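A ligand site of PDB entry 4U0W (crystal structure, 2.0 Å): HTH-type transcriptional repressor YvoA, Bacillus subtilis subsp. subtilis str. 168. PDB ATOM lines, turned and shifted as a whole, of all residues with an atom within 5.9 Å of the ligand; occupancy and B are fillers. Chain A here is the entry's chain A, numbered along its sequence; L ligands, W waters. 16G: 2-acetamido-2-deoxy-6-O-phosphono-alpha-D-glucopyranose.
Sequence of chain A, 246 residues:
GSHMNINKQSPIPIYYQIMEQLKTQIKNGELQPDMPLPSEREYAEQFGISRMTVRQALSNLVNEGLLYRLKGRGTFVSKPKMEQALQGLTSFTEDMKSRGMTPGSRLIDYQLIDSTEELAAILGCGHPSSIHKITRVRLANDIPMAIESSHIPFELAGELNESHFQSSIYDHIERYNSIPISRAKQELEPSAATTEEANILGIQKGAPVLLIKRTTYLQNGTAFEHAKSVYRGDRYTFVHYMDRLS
The backbone NH (N) of Arg 136 lies within hydrogen-bond range of the backbone carbonyl oxygen (O) of Glu 148, 2.9 Å away.
The guanidinium group (NH1) of Arg 138 lies within salt-bridge range of the side-chain carboxylate (OE1) of Glu 148, at 2.8 Å.
The side-chain hydroxyl (OG) of Ser 150 sits at hydrogen-bond distance from the side-chain carboxylate (OE1) of Glu 225.
OG of Ser 168 is in hydrogen-bond range of N of Asp 171 (3.0 Å).
NH2 of Arg 136 lies within hydrogen-bond range of O of Ser 167, at 3.2 Å.
NH2 of Arg 136 lies within hydrogen-bond range of OG of Ser 105 (3.4 Å).
O of Ala 227 lies within hydrogen-bond range of N of Arg 214 (2.8 Å).
OG1 of Thr 90 sits at hydrogen-bond distance from OD1 of Asp 95 (2.5 Å).
N of Thr 93 lies within hydrogen-bond range of O3P of the ligand (3.1 Å).
The side-chain hydroxyl of Thr 93 sits at hydrogen-bond distance from an oxygen (O3P) of the ligand, 2.6 Å away.
The side-chain carboxylate of Glu 148 sits at hydrogen-bond distance from an oxygen (O1) of the ligand (2.6 Å).
The side-chain carboxylate (OE1) of Glu 225 lies within hydrogen-bond range of an oxygen (O4) of the ligand, at 2.6 Å.
An oxygen (O2P) of the ligand lies within hydrogen-bond range of the side-chain hydroxyl (OG) of Ser 168 (2.6 Å).
An oxygen (O1P) of the ligand lies within salt-bridge range of the guanidinium group (NH1) of Arg 136 (2.7 Å).
The guanidinium group of Arg 138 lies within salt-bridge range of an oxygen (O3P) of the ligand, at 2.7 Å.
The backbone NH of Ile 169 lies within hydrogen-bond range of an oxygen (O1P) of the ligand, 2.7 Å away.
The backbone NH (N) of Tyr 170 lies within hydrogen-bond range of an oxygen (O2P) of the ligand (2.9 Å).
O5 of the ligand is in hydrogen-bond range of N of Phe 92 (3.1 Å).
The side-chain hydroxyl (OH) of Tyr 231 sits at hydrogen-bond distance from an oxygen (O1) of the ligand, at 3.2 Å.
The guanidinium group (NE) of Arg 214 is in hydrogen-bond range of an oxygen (O7) of the ligand (3.2 Å).
Water W3 lies within hydrogen-bond range of an oxygen (O4) of the ligand (2.7 Å), the side-chain carboxylate of Glu 148 (2.8 Å) and the guanidinium group of Arg 136 (3.1 Å).
Water W1 lies within hydrogen-bond range of OD2 of Asp 95, OH of Tyr 231 and O1 of the ligand.
Thr 90 touches the ligand.
Ser 91 touches the ligand (CB to O2P, 3.2 Å).
Ser 167 touches the ligand.
Gln 186 touches the ligand.
CG2 of Ile 212 touches C8 of the ligand, at 3.6 Å.
Ala 227 touches the ligand.
Ser 229 touches the ligand (OG to C8, 3.8 Å).
Hydrophobic or aromatic side chains that line the ligand: Phe 92, Ile 169, Tyr 170, Ile 212, Ala 227 and Tyr 231.
Of the 26 residues printed, 18 come within 4 Å of the ligand.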
ATOM      1  N   THR A  90       5.224  37.063  21.908  1.00  0.00           N
ATOM      2  CA  THR A  90       4.245  36.172  21.286  1.00  0.00           C
ATOM      3  C   THR A  90       4.886  34.834  20.932  1.00  0.00           C
ATOM      4  O   THR A  90       6.106  34.729  20.831  1.00  0.00           O
ATOM      5  CB  THR A  90       3.645  36.763  19.990  1.00  0.00           C
ATOM      6  OG1 THR A  90       4.692  36.997  19.044  1.00  0.00           O
ATOM      7  CG2 THR A  90       2.881  38.078  20.247  1.00  0.00           C
ATOM      8  N   SER A  91       4.037  33.841  20.719  1.00  0.00           N
ATOM      9  CA  SER A  91       4.464  32.545  20.209  1.00  0.00           C
ATOM     10  C   SER A  91       4.422  32.531  18.699  1.00  0.00           C
ATOM     11  O   SER A  91       3.762  33.381  18.083  1.00  0.00           O
ATOM     12  CB  SER A  91       3.572  31.428  20.756  1.00  0.00           C
ATOM     13  OG  SER A  91       2.249  31.522  20.233  1.00  0.00           O
ATOM     14  N   PHE A  92       5.103  31.552  18.114  1.00  0.00           N
ATOM     15  CA  PHE A  92       5.030  31.342  16.676  1.00  0.00           C
ATOM     16  C   PHE A  92       3.571  31.128  16.261  1.00  0.00           C
ATOM     17  O   PHE A  92       3.115  31.684  15.271  1.00  0.00           O
ATOM     18  CB  PHE A  92       5.883  30.136  16.251  1.00  0.00           C
ATOM     19  CG  PHE A  92       5.939  29.929  14.754  1.00  0.00           C
ATOM     20  CD1 PHE A  92       6.835  30.636  13.961  1.00  0.00           C
ATOM     21  CD2 PHE A  92       5.099  29.006  14.140  1.00  0.00           C
ATOM     22  CE1 PHE A  92       6.895  30.442  12.580  1.00  0.00           C
ATOM     23  CE2 PHE A  92       5.161  28.798  12.762  1.00  0.00           C
ATOM     24  CZ  PHE A  92       6.054  29.523  11.983  1.00  0.00           C
ATOM     25  N   THR A  93       2.854  30.327  17.049  1.00  0.00           N
ATOM     26  CA  THR A  93       1.454  30.012  16.791  1.00  0.00           C
ATOM     27  C   THR A  93       0.621  31.292  16.726  1.00  0.00           C
ATOM     28  O   THR A  93      -0.103  31.497  15.771  1.00  0.00           O
ATOM     29  CB  THR A  93       0.893  29.070  17.861  1.00  0.00           C
ATOM     30  OG1 THR A  93       1.569  27.816  17.746  1.00  0.00           O
ATOM     31  CG2 THR A  93      -0.599  28.820  17.667  1.00  0.00           C
ATOM     32  N   GLU A  94       0.754  32.131  17.754  1.00  0.00           N
ATOM     33  CA  GLU A  94       0.091  33.434  17.782  1.00  0.00           C
ATOM     34  C   GLU A  94       0.462  34.289  16.549  1.00  0.00           C
ATOM     35  O   GLU A  94      -0.423  34.898  15.927  1.00  0.00           O
ATOM     36  CB  GLU A  94       0.430  34.168  19.081  1.00  0.00           C
ATOM     37  CG  GLU A  94      -0.252  33.576  20.327  1.00  0.00           C
ATOM     38  CD  GLU A  94       0.290  34.117  21.650  1.00  0.00           C
ATOM     39  OE1 GLU A  94      -0.416  34.008  22.680  1.00  0.00           O
ATOM     40  OE2 GLU A  94       1.428  34.629  21.667  1.00  0.00           O
ATOM     41  N   ASP A  95       1.750  34.329  16.193  1.00  0.00           N
ATOM     42  CA  ASP A  95       2.219  35.101  15.032  1.00  0.00           C
ATOM     43  C   ASP A  95       1.500  34.712  13.736  1.00  0.00           C
ATOM     44  O   ASP A  95       1.010  35.570  12.996  1.00  0.00           O
ATOM     45  CB  ASP A  95       3.732  34.924  14.808  1.00  0.00           C
ATOM     46  CG  ASP A  95       4.575  35.555  15.902  1.00  0.00           C
ATOM     47  OD1 ASP A  95       4.087  36.447  16.629  1.00  0.00           O
ATOM     48  OD2 ASP A  95       5.747  35.154  16.024  1.00  0.00           O
ATOM     49  N   SER A 105       4.649  22.492  12.776  1.00  0.00           N
ATOM     50  CA  SER A 105       5.986  22.123  13.220  1.00  0.00           C
ATOM     51  C   SER A 105       6.400  20.767  12.651  1.00  0.00           C
ATOM     52  O   SER A 105       5.558  19.896  12.417  1.00  0.00           O
ATOM     53  CB  SER A 105       6.086  22.092  14.743  1.00  0.00           C
ATOM     54  OG  SER A 105       5.974  23.385  15.312  1.00  0.00           O
ATOM     55  N   ARG A 136      12.598  22.182  16.702  1.00  0.00           N
ATOM     56  CA  ARG A 136      11.579  22.074  15.671  1.00  0.00           C
ATOM     57  C   ARG A 136      11.831  23.013  14.478  1.00  0.00           C
ATOM     58  O   ARG A 136      12.334  24.128  14.663  1.00  0.00           O
ATOM     59  CB  ARG A 136      10.193  22.375  16.235  1.00  0.00           C
ATOM     60  CG  ARG A 136       9.803  21.551  17.460  1.00  0.00           C
ATOM     61  CD  ARG A 136       8.437  21.949  17.950  1.00  0.00           C
ATOM     62  NE  ARG A 136       8.447  23.255  18.612  1.00  0.00           N
ATOM     63  CZ  ARG A 136       7.363  23.936  18.958  1.00  0.00           C
ATOM     64  NH1 ARG A 136       7.476  25.111  19.572  1.00  0.00           N
ATOM     65  NH2 ARG A 136       6.157  23.443  18.697  1.00  0.00           N
ATOM     66  N   ARG A 138       9.725  25.412  12.341  1.00  0.00           N
ATOM     67  CA  ARG A 138       8.392  26.015  12.420  1.00  0.00           C
ATOM     68  C   ARG A 138       7.932  26.373  11.000  1.00  0.00           C
ATOM     69  O   ARG A 138       8.685  26.932  10.221  1.00  0.00           O
ATOM     70  CB  ARG A 138       8.394  27.258  13.320  1.00  0.00           C
ATOM     71  CG  ARG A 138       9.095  27.064  14.657  1.00  0.00           C
ATOM     72  CD  ARG A 138       8.555  25.870  15.424  1.00  0.00           C
ATOM     73  NE  ARG A 138       7.105  25.923  15.703  1.00  0.00           N
ATOM     74  CZ  ARG A 138       6.546  26.622  16.695  1.00  0.00           C
ATOM     75  NH1 ARG A 138       7.305  27.390  17.469  1.00  0.00           N
ATOM     76  NH2 ARG A 138       5.229  26.570  16.898  1.00  0.00           N
ATOM     77  N   GLU A 148      13.947  26.400  15.625  1.00  0.00           N
ATOM     78  CA  GLU A 148      14.013  26.809  17.006  1.00  0.00           C
ATOM     79  C   GLU A 148      14.464  25.657  17.911  1.00  0.00           C
ATOM     80  O   GLU A 148      14.039  24.528  17.733  1.00  0.00           O
ATOM     81  CB  GLU A 148      12.654  27.329  17.475  1.00  0.00           C
ATOM     82  CG  GLU A 148      12.146  28.518  16.649  1.00  0.00           C
ATOM     83  CD  GLU A 148      10.735  28.921  17.035  1.00  0.00           C
ATOM     84  OE1 GLU A 148      10.016  28.059  17.563  1.00  0.00           O
ATOM     85  OE2 GLU A 148      10.363  30.099  16.810  1.00  0.00           O
ATOM     86  N   SER A 150      14.439  24.983  21.823  1.00  0.00           N
ATOM     87  CA  SER A 150      13.980  25.550  23.088  1.00  0.00           C
ATOM     88  C   SER A 150      14.419  24.690  24.276  1.00  0.00           C
ATOM     89  O   SER A 150      14.226  23.483  24.246  1.00  0.00           O
ATOM     90  CB  SER A 150      12.462  25.699  23.104  1.00  0.00           C
ATOM     91  OG  SER A 150      12.061  26.311  24.332  1.00  0.00           O
ATOM     92  N   HIS A 164       2.436  17.681  21.820  1.00  0.00           N
ATOM     93  CA  HIS A 164       2.876  18.979  22.334  1.00  0.00           C
ATOM     94  C   HIS A 164       3.691  19.698  21.274  1.00  0.00           C
ATOM     95  O   HIS A 164       3.475  20.885  21.032  1.00  0.00           O
ATOM     96  CB  HIS A 164       3.712  18.824  23.604  1.00  0.00           C
ATOM     97  CG  HIS A 164       2.943  18.328  24.794  1.00  0.00           C
ATOM     98  ND1 HIS A 164       3.017  17.021  25.234  1.00  0.00           N
ATOM     99  CD2 HIS A 164       2.094  18.962  25.638  1.00  0.00           C
ATOM    100  CE1 HIS A 164       2.255  16.875  26.305  1.00  0.00           C
ATOM    101  NE2 HIS A 164       1.680  18.043  26.569  1.00  0.00           N
ATOM    102  N   SER A 167       1.794  21.292  18.464  1.00  0.00           N
ATOM    103  CA  SER A 167       0.930  22.377  18.885  1.00  0.00           C
ATOM    104  C   SER A 167       1.796  23.522  19.421  1.00  0.00           C
ATOM    105  O   SER A 167       2.964  23.629  19.067  1.00  0.00           O
ATOM    106  CB  SER A 167      -0.065  21.897  19.936  1.00  0.00           C
ATOM    107  OG  SER A 167      -0.946  22.939  20.313  1.00  0.00           O
ATOM    108  N   SER A 168       1.220  24.342  20.285  1.00  0.00           N
ATOM    109  CA  SER A 168       1.931  25.497  20.822  1.00  0.00           C
ATOM    110  C   SER A 168       2.542  25.203  22.182  1.00  0.00           C
ATOM    111  O   SER A 168       1.834  24.909  23.146  1.00  0.00           O
ATOM    112  CB  SER A 168       0.991  26.698  20.917  1.00  0.00           C
ATOM    113  OG  SER A 168       1.503  27.672  21.816  1.00  0.00           O
ATOM    114  N   ILE A 169       3.866  25.292  22.261  1.00  0.00           N
ATOM    115  CA  ILE A 169       4.547  25.123  23.532  1.00  0.00           C
ATOM    116  C   ILE A 169       4.176  26.242  24.535  1.00  0.00           C
ATOM    117  O   ILE A 169       4.009  25.965  25.720  1.00  0.00           O
ATOM    118  CB  ILE A 169       6.085  25.075  23.334  1.00  0.00           C
ATOM    119  CG1 ILE A 169       6.450  23.794  22.586  1.00  0.00           C
ATOM    120  CG2 ILE A 169       6.825  25.123  24.666  1.00  0.00           C
ATOM    121  CD1 ILE A 169       6.125  22.535  23.385  1.00  0.00           C
ATOM    122  N   TYR A 170       4.028  27.478  24.072  1.00  0.00           N
ATOM    123  CA  TYR A 170       3.709  28.568  25.008  1.00  0.00           C
ATOM    124  C   TYR A 170       2.327  28.343  25.649  1.00  0.00           C
ATOM    125  O   TYR A 170       2.139  28.616  26.839  1.00  0.00           O
ATOM    126  CB  TYR A 170       3.752  29.936  24.294  1.00  0.00           C
ATOM    127  CG  TYR A 170       5.148  30.542  24.196  1.00  0.00           C
ATOM    128  CD1 TYR A 170       6.287  29.773  24.471  1.00  0.00           C
ATOM    129  CD2 TYR A 170       5.318  31.872  23.854  1.00  0.00           C
ATOM    130  CE1 TYR A 170       7.565  30.344  24.375  1.00  0.00           C
ATOM    131  CE2 TYR A 170       6.584  32.447  23.756  1.00  0.00           C
ATOM    132  CZ  TYR A 170       7.702  31.679  24.017  1.00  0.00           C
ATOM    133  OH  TYR A 170       8.956  32.267  23.922  1.00  0.00           O
ATOM    134  N   ASP A 171       1.376  27.857  24.848  1.00  0.00           N
ATOM    135  CA  ASP A 171       0.049  27.543  25.352  1.00  0.00           C
ATOM    136  C   ASP A 171       0.112  26.477  26.454  1.00  0.00           C
ATOM    137  O   ASP A 171      -0.491  26.618  27.522  1.00  0.00           O
ATOM    138  CB  ASP A 171      -0.855  27.071  24.226  1.00  0.00           C
ATOM    139  CG  ASP A 171      -2.297  27.398  24.473  1.00  0.00           C
ATOM    140  OD1 ASP A 171      -2.640  28.594  24.364  1.00  0.00           O
ATOM    141  OD2 ASP A 171      -3.075  26.486  24.802  1.00  0.00           O
ATOM    142  N   GLN A 186      15.718  39.172  24.300  1.00  0.00           N
ATOM    143  CA  GLN A 186      16.196  38.573  23.043  1.00  0.00           C
ATOM    144  C   GLN A 186      17.506  39.200  22.563  1.00  0.00           C
ATOM    145  O   GLN A 186      17.710  40.402  22.719  1.00  0.00           O
ATOM    146  CB  GLN A 186      15.148  38.696  21.923  1.00  0.00           C
ATOM    147  CG  GLN A 186      14.260  37.486  21.787  1.00  0.00           C
ATOM    148  CD  GLN A 186      13.365  37.510  20.567  1.00  0.00           C
ATOM    149  OE1 GLN A 186      12.719  36.503  20.261  1.00  0.00           O
ATOM    150  NE2 GLN A 186      13.305  38.645  19.853  1.00  0.00           N
ATOM    151  N   ILE A 212      18.686  34.190  16.752  1.00  0.00           N
ATOM    152  CA  ILE A 212      17.960  34.773  17.851  1.00  0.00           C
ATOM    153  C   ILE A 212      18.162  33.933  19.117  1.00  0.00           C
ATOM    154  O   ILE A 212      17.994  32.727  19.071  1.00  0.00           O
ATOM    155  CB  ILE A 212      16.456  34.908  17.546  1.00  0.00           C
ATOM    156  CG1 ILE A 212      16.263  35.661  16.217  1.00  0.00           C
ATOM    157  CG2 ILE A 212      15.768  35.641  18.690  1.00  0.00           C
ATOM    158  CD1 ILE A 212      14.781  35.821  15.748  1.00  0.00           C
ATOM    159  N   LYS A 213      18.515  34.586  20.215  1.00  0.00           N
ATOM    160  CA  LYS A 213      18.587  33.932  21.527  1.00  0.00           C
ATOM    161  C   LYS A 213      17.542  34.568  22.437  1.00  0.00           C
ATOM    162  O   LYS A 213      17.581  35.780  22.671  1.00  0.00           O
ATOM    163  CB  LYS A 213      19.992  34.063  22.129  1.00  0.00           C
ATOM    164  CG  LYS A 213      20.312  33.151  23.281  1.00  0.00           C
ATOM    165  CD  LYS A 213      21.633  33.557  23.929  1.00  0.00           C
ATOM    166  CE  LYS A 213      22.774  33.579  22.918  1.00  0.00           C
ATOM    167  NZ  LYS A 213      24.078  33.895  23.574  1.00  0.00           N
ATOM    168  N   ARG A 214      16.587  33.771  22.921  1.00  0.00           N
ATOM    169  CA  ARG A 214      15.500  34.279  23.763  1.00  0.00           C
ATOM    170  C   ARG A 214      15.449  33.631  25.162  1.00  0.00           C
ATOM    171  O   ARG A 214      15.443  32.413  25.287  1.00  0.00           O
ATOM    172  CB  ARG A 214      14.149  34.058  23.077  1.00  0.00           C
ATOM    173  CG  ARG A 214      12.963  34.449  23.964  1.00  0.00           C
ATOM    174  CD  ARG A 214      11.611  34.169  23.309  1.00  0.00           C
ATOM    175  NE  ARG A 214      11.342  35.027  22.143  1.00  0.00           N
ATOM    176  CZ  ARG A 214      10.165  35.120  21.532  1.00  0.00           C
ATOM    177  NH1 ARG A 214       9.129  34.427  21.989  1.00  0.00           N
ATOM    178  NH2 ARG A 214      10.016  35.907  20.471  1.00  0.00           N
ATOM    179  N   THR A 216      12.871  33.524  28.308  1.00  0.00           N
ATOM    180  CA  THR A 216      11.463  33.861  28.443  1.00  0.00           C
ATOM    181  C   THR A 216      11.007  33.605  29.880  1.00  0.00           C
ATOM    182  O   THR A 216      11.429  32.609  30.493  1.00  0.00           O
ATOM    183  CB  THR A 216      10.630  33.034  27.446  1.00  0.00           C
ATOM    184  OG1 THR A 216      11.394  32.835  26.258  1.00  0.00           O
ATOM    185  CG2 THR A 216       9.324  33.748  27.099  1.00  0.00           C
ATOM    186  N   GLU A 225      12.207  29.371  29.732  1.00  0.00           N
ATOM    187  CA  GLU A 225      12.711  29.040  28.399  1.00  0.00           C
ATOM    188  C   GLU A 225      14.022  29.785  28.106  1.00  0.00           C
ATOM    189  O   GLU A 225      14.171  30.967  28.411  1.00  0.00           O
ATOM    190  CB  GLU A 225      11.687  29.373  27.305  1.00  0.00           C
ATOM    191  CG  GLU A 225      12.193  29.081  25.886  1.00  0.00           C
ATOM    192  CD  GLU A 225      11.236  29.547  24.807  1.00  0.00           C
ATOM    193  OE1 GLU A 225      10.951  28.739  23.877  1.00  0.00           O
ATOM    194  OE2 GLU A 225      10.795  30.722  24.875  1.00  0.00           O
ATOM    195  N   ALA A 227      15.920  29.783  24.456  1.00  0.00           N
ATOM    196  CA  ALA A 227      15.804  29.261  23.104  1.00  0.00           C
ATOM    197  C   ALA A 227      16.794  29.943  22.162  1.00  0.00           C
ATOM    198  O   ALA A 227      17.098  31.123  22.304  1.00  0.00           O
ATOM    199  CB  ALA A 227      14.400  29.432  22.588  1.00  0.00           C
ATOM    200  N   SER A 229      17.459  30.266  17.953  1.00  0.00           N
ATOM    201  CA  SER A 229      16.705  30.066  16.738  1.00  0.00           C
ATOM    202  C   SER A 229      17.403  30.679  15.535  1.00  0.00           C
ATOM    203  O   SER A 229      18.225  31.593  15.687  1.00  0.00           O
ATOM    204  CB  SER A 229      15.298  30.663  16.849  1.00  0.00           C
ATOM    205  OG  SER A 229      14.655  30.297  18.053  1.00  0.00           O
ATOM    206  N   TYR A 231      16.051  32.317  11.956  1.00  0.00           N
ATOM    207  CA  TYR A 231      14.924  32.786  11.145  1.00  0.00           C
ATOM    208  C   TYR A 231      15.376  33.170   9.726  1.00  0.00           C
ATOM    209  O   TYR A 231      16.386  33.851   9.555  1.00  0.00           O
ATOM    210  CB  TYR A 231      14.252  33.981  11.825  1.00  0.00           C
ATOM    211  CG  TYR A 231      13.199  33.570  12.809  1.00  0.00           C
ATOM    212  CD1 TYR A 231      13.537  32.838  13.957  1.00  0.00           C
ATOM    213  CD2 TYR A 231      11.860  33.867  12.595  1.00  0.00           C
ATOM    214  CE1 TYR A 231      12.572  32.431  14.857  1.00  0.00           C
ATOM    215  CE2 TYR A 231      10.880  33.479  13.490  1.00  0.00           C
ATOM    216  CZ  TYR A 231      11.244  32.756  14.625  1.00  0.00           C
ATOM    217  OH  TYR A 231      10.285  32.363  15.516  1.00  0.00           O
HETATM  218  C1  16G L   1       8.444  31.979  19.273  1.00  0.00           C
HETATM  219  C2  16G L   1       9.820  31.999  19.933  1.00  0.00           C
HETATM  220  C3  16G L   1      10.282  30.656  20.360  1.00  0.00           C
HETATM  221  C4  16G L   1       9.235  29.976  21.162  1.00  0.00           C
HETATM  222  C5  16G L   1       8.042  29.796  20.245  1.00  0.00           C
HETATM  223  C6  16G L   1       6.970  28.948  20.858  1.00  0.00           C
HETATM  224  C7  16G L   1      12.086  32.993  19.208  1.00  0.00           C
HETATM  225  C8  16G L   1      12.845  33.678  18.081  1.00  0.00           C
HETATM  226  N2  16G L   1      10.716  32.646  18.977  1.00  0.00           N
HETATM  227  O1  16G L   1       8.551  31.458  18.003  1.00  0.00           O
HETATM  228  O3  16G L   1      11.452  30.741  21.203  1.00  0.00           O
HETATM  229  O4  16G L   1       9.690  28.694  21.634  1.00  0.00           O
HETATM  230  O5  16G L   1       7.474  31.114  19.984  1.00  0.00           O
HETATM  231  O6  16G L   1       5.948  28.861  19.858  1.00  0.00           O
HETATM  232  O7  16G L   1      12.645  32.757  20.256  1.00  0.00           O
HETATM  233  P   16G L   1       4.731  27.839  20.029  1.00  0.00           P
HETATM  234  O1P 16G L   1       5.236  26.413  20.192  1.00  0.00           O
HETATM  235  O2P 16G L   1       3.970  28.264  21.268  1.00  0.00           O
HETATM  236  O3P 16G L   1       3.902  27.955  18.768  1.00  0.00           O
HETATM  237  O   HOH W   1       8.017  33.929  16.247  1.00  0.00           O
HETATM  238  O   HOH W   2      15.050  31.837  20.009  1.00  0.00           O
HETATM  239  O   HOH W   3      10.141  26.668  19.938  1.00  0.00           O
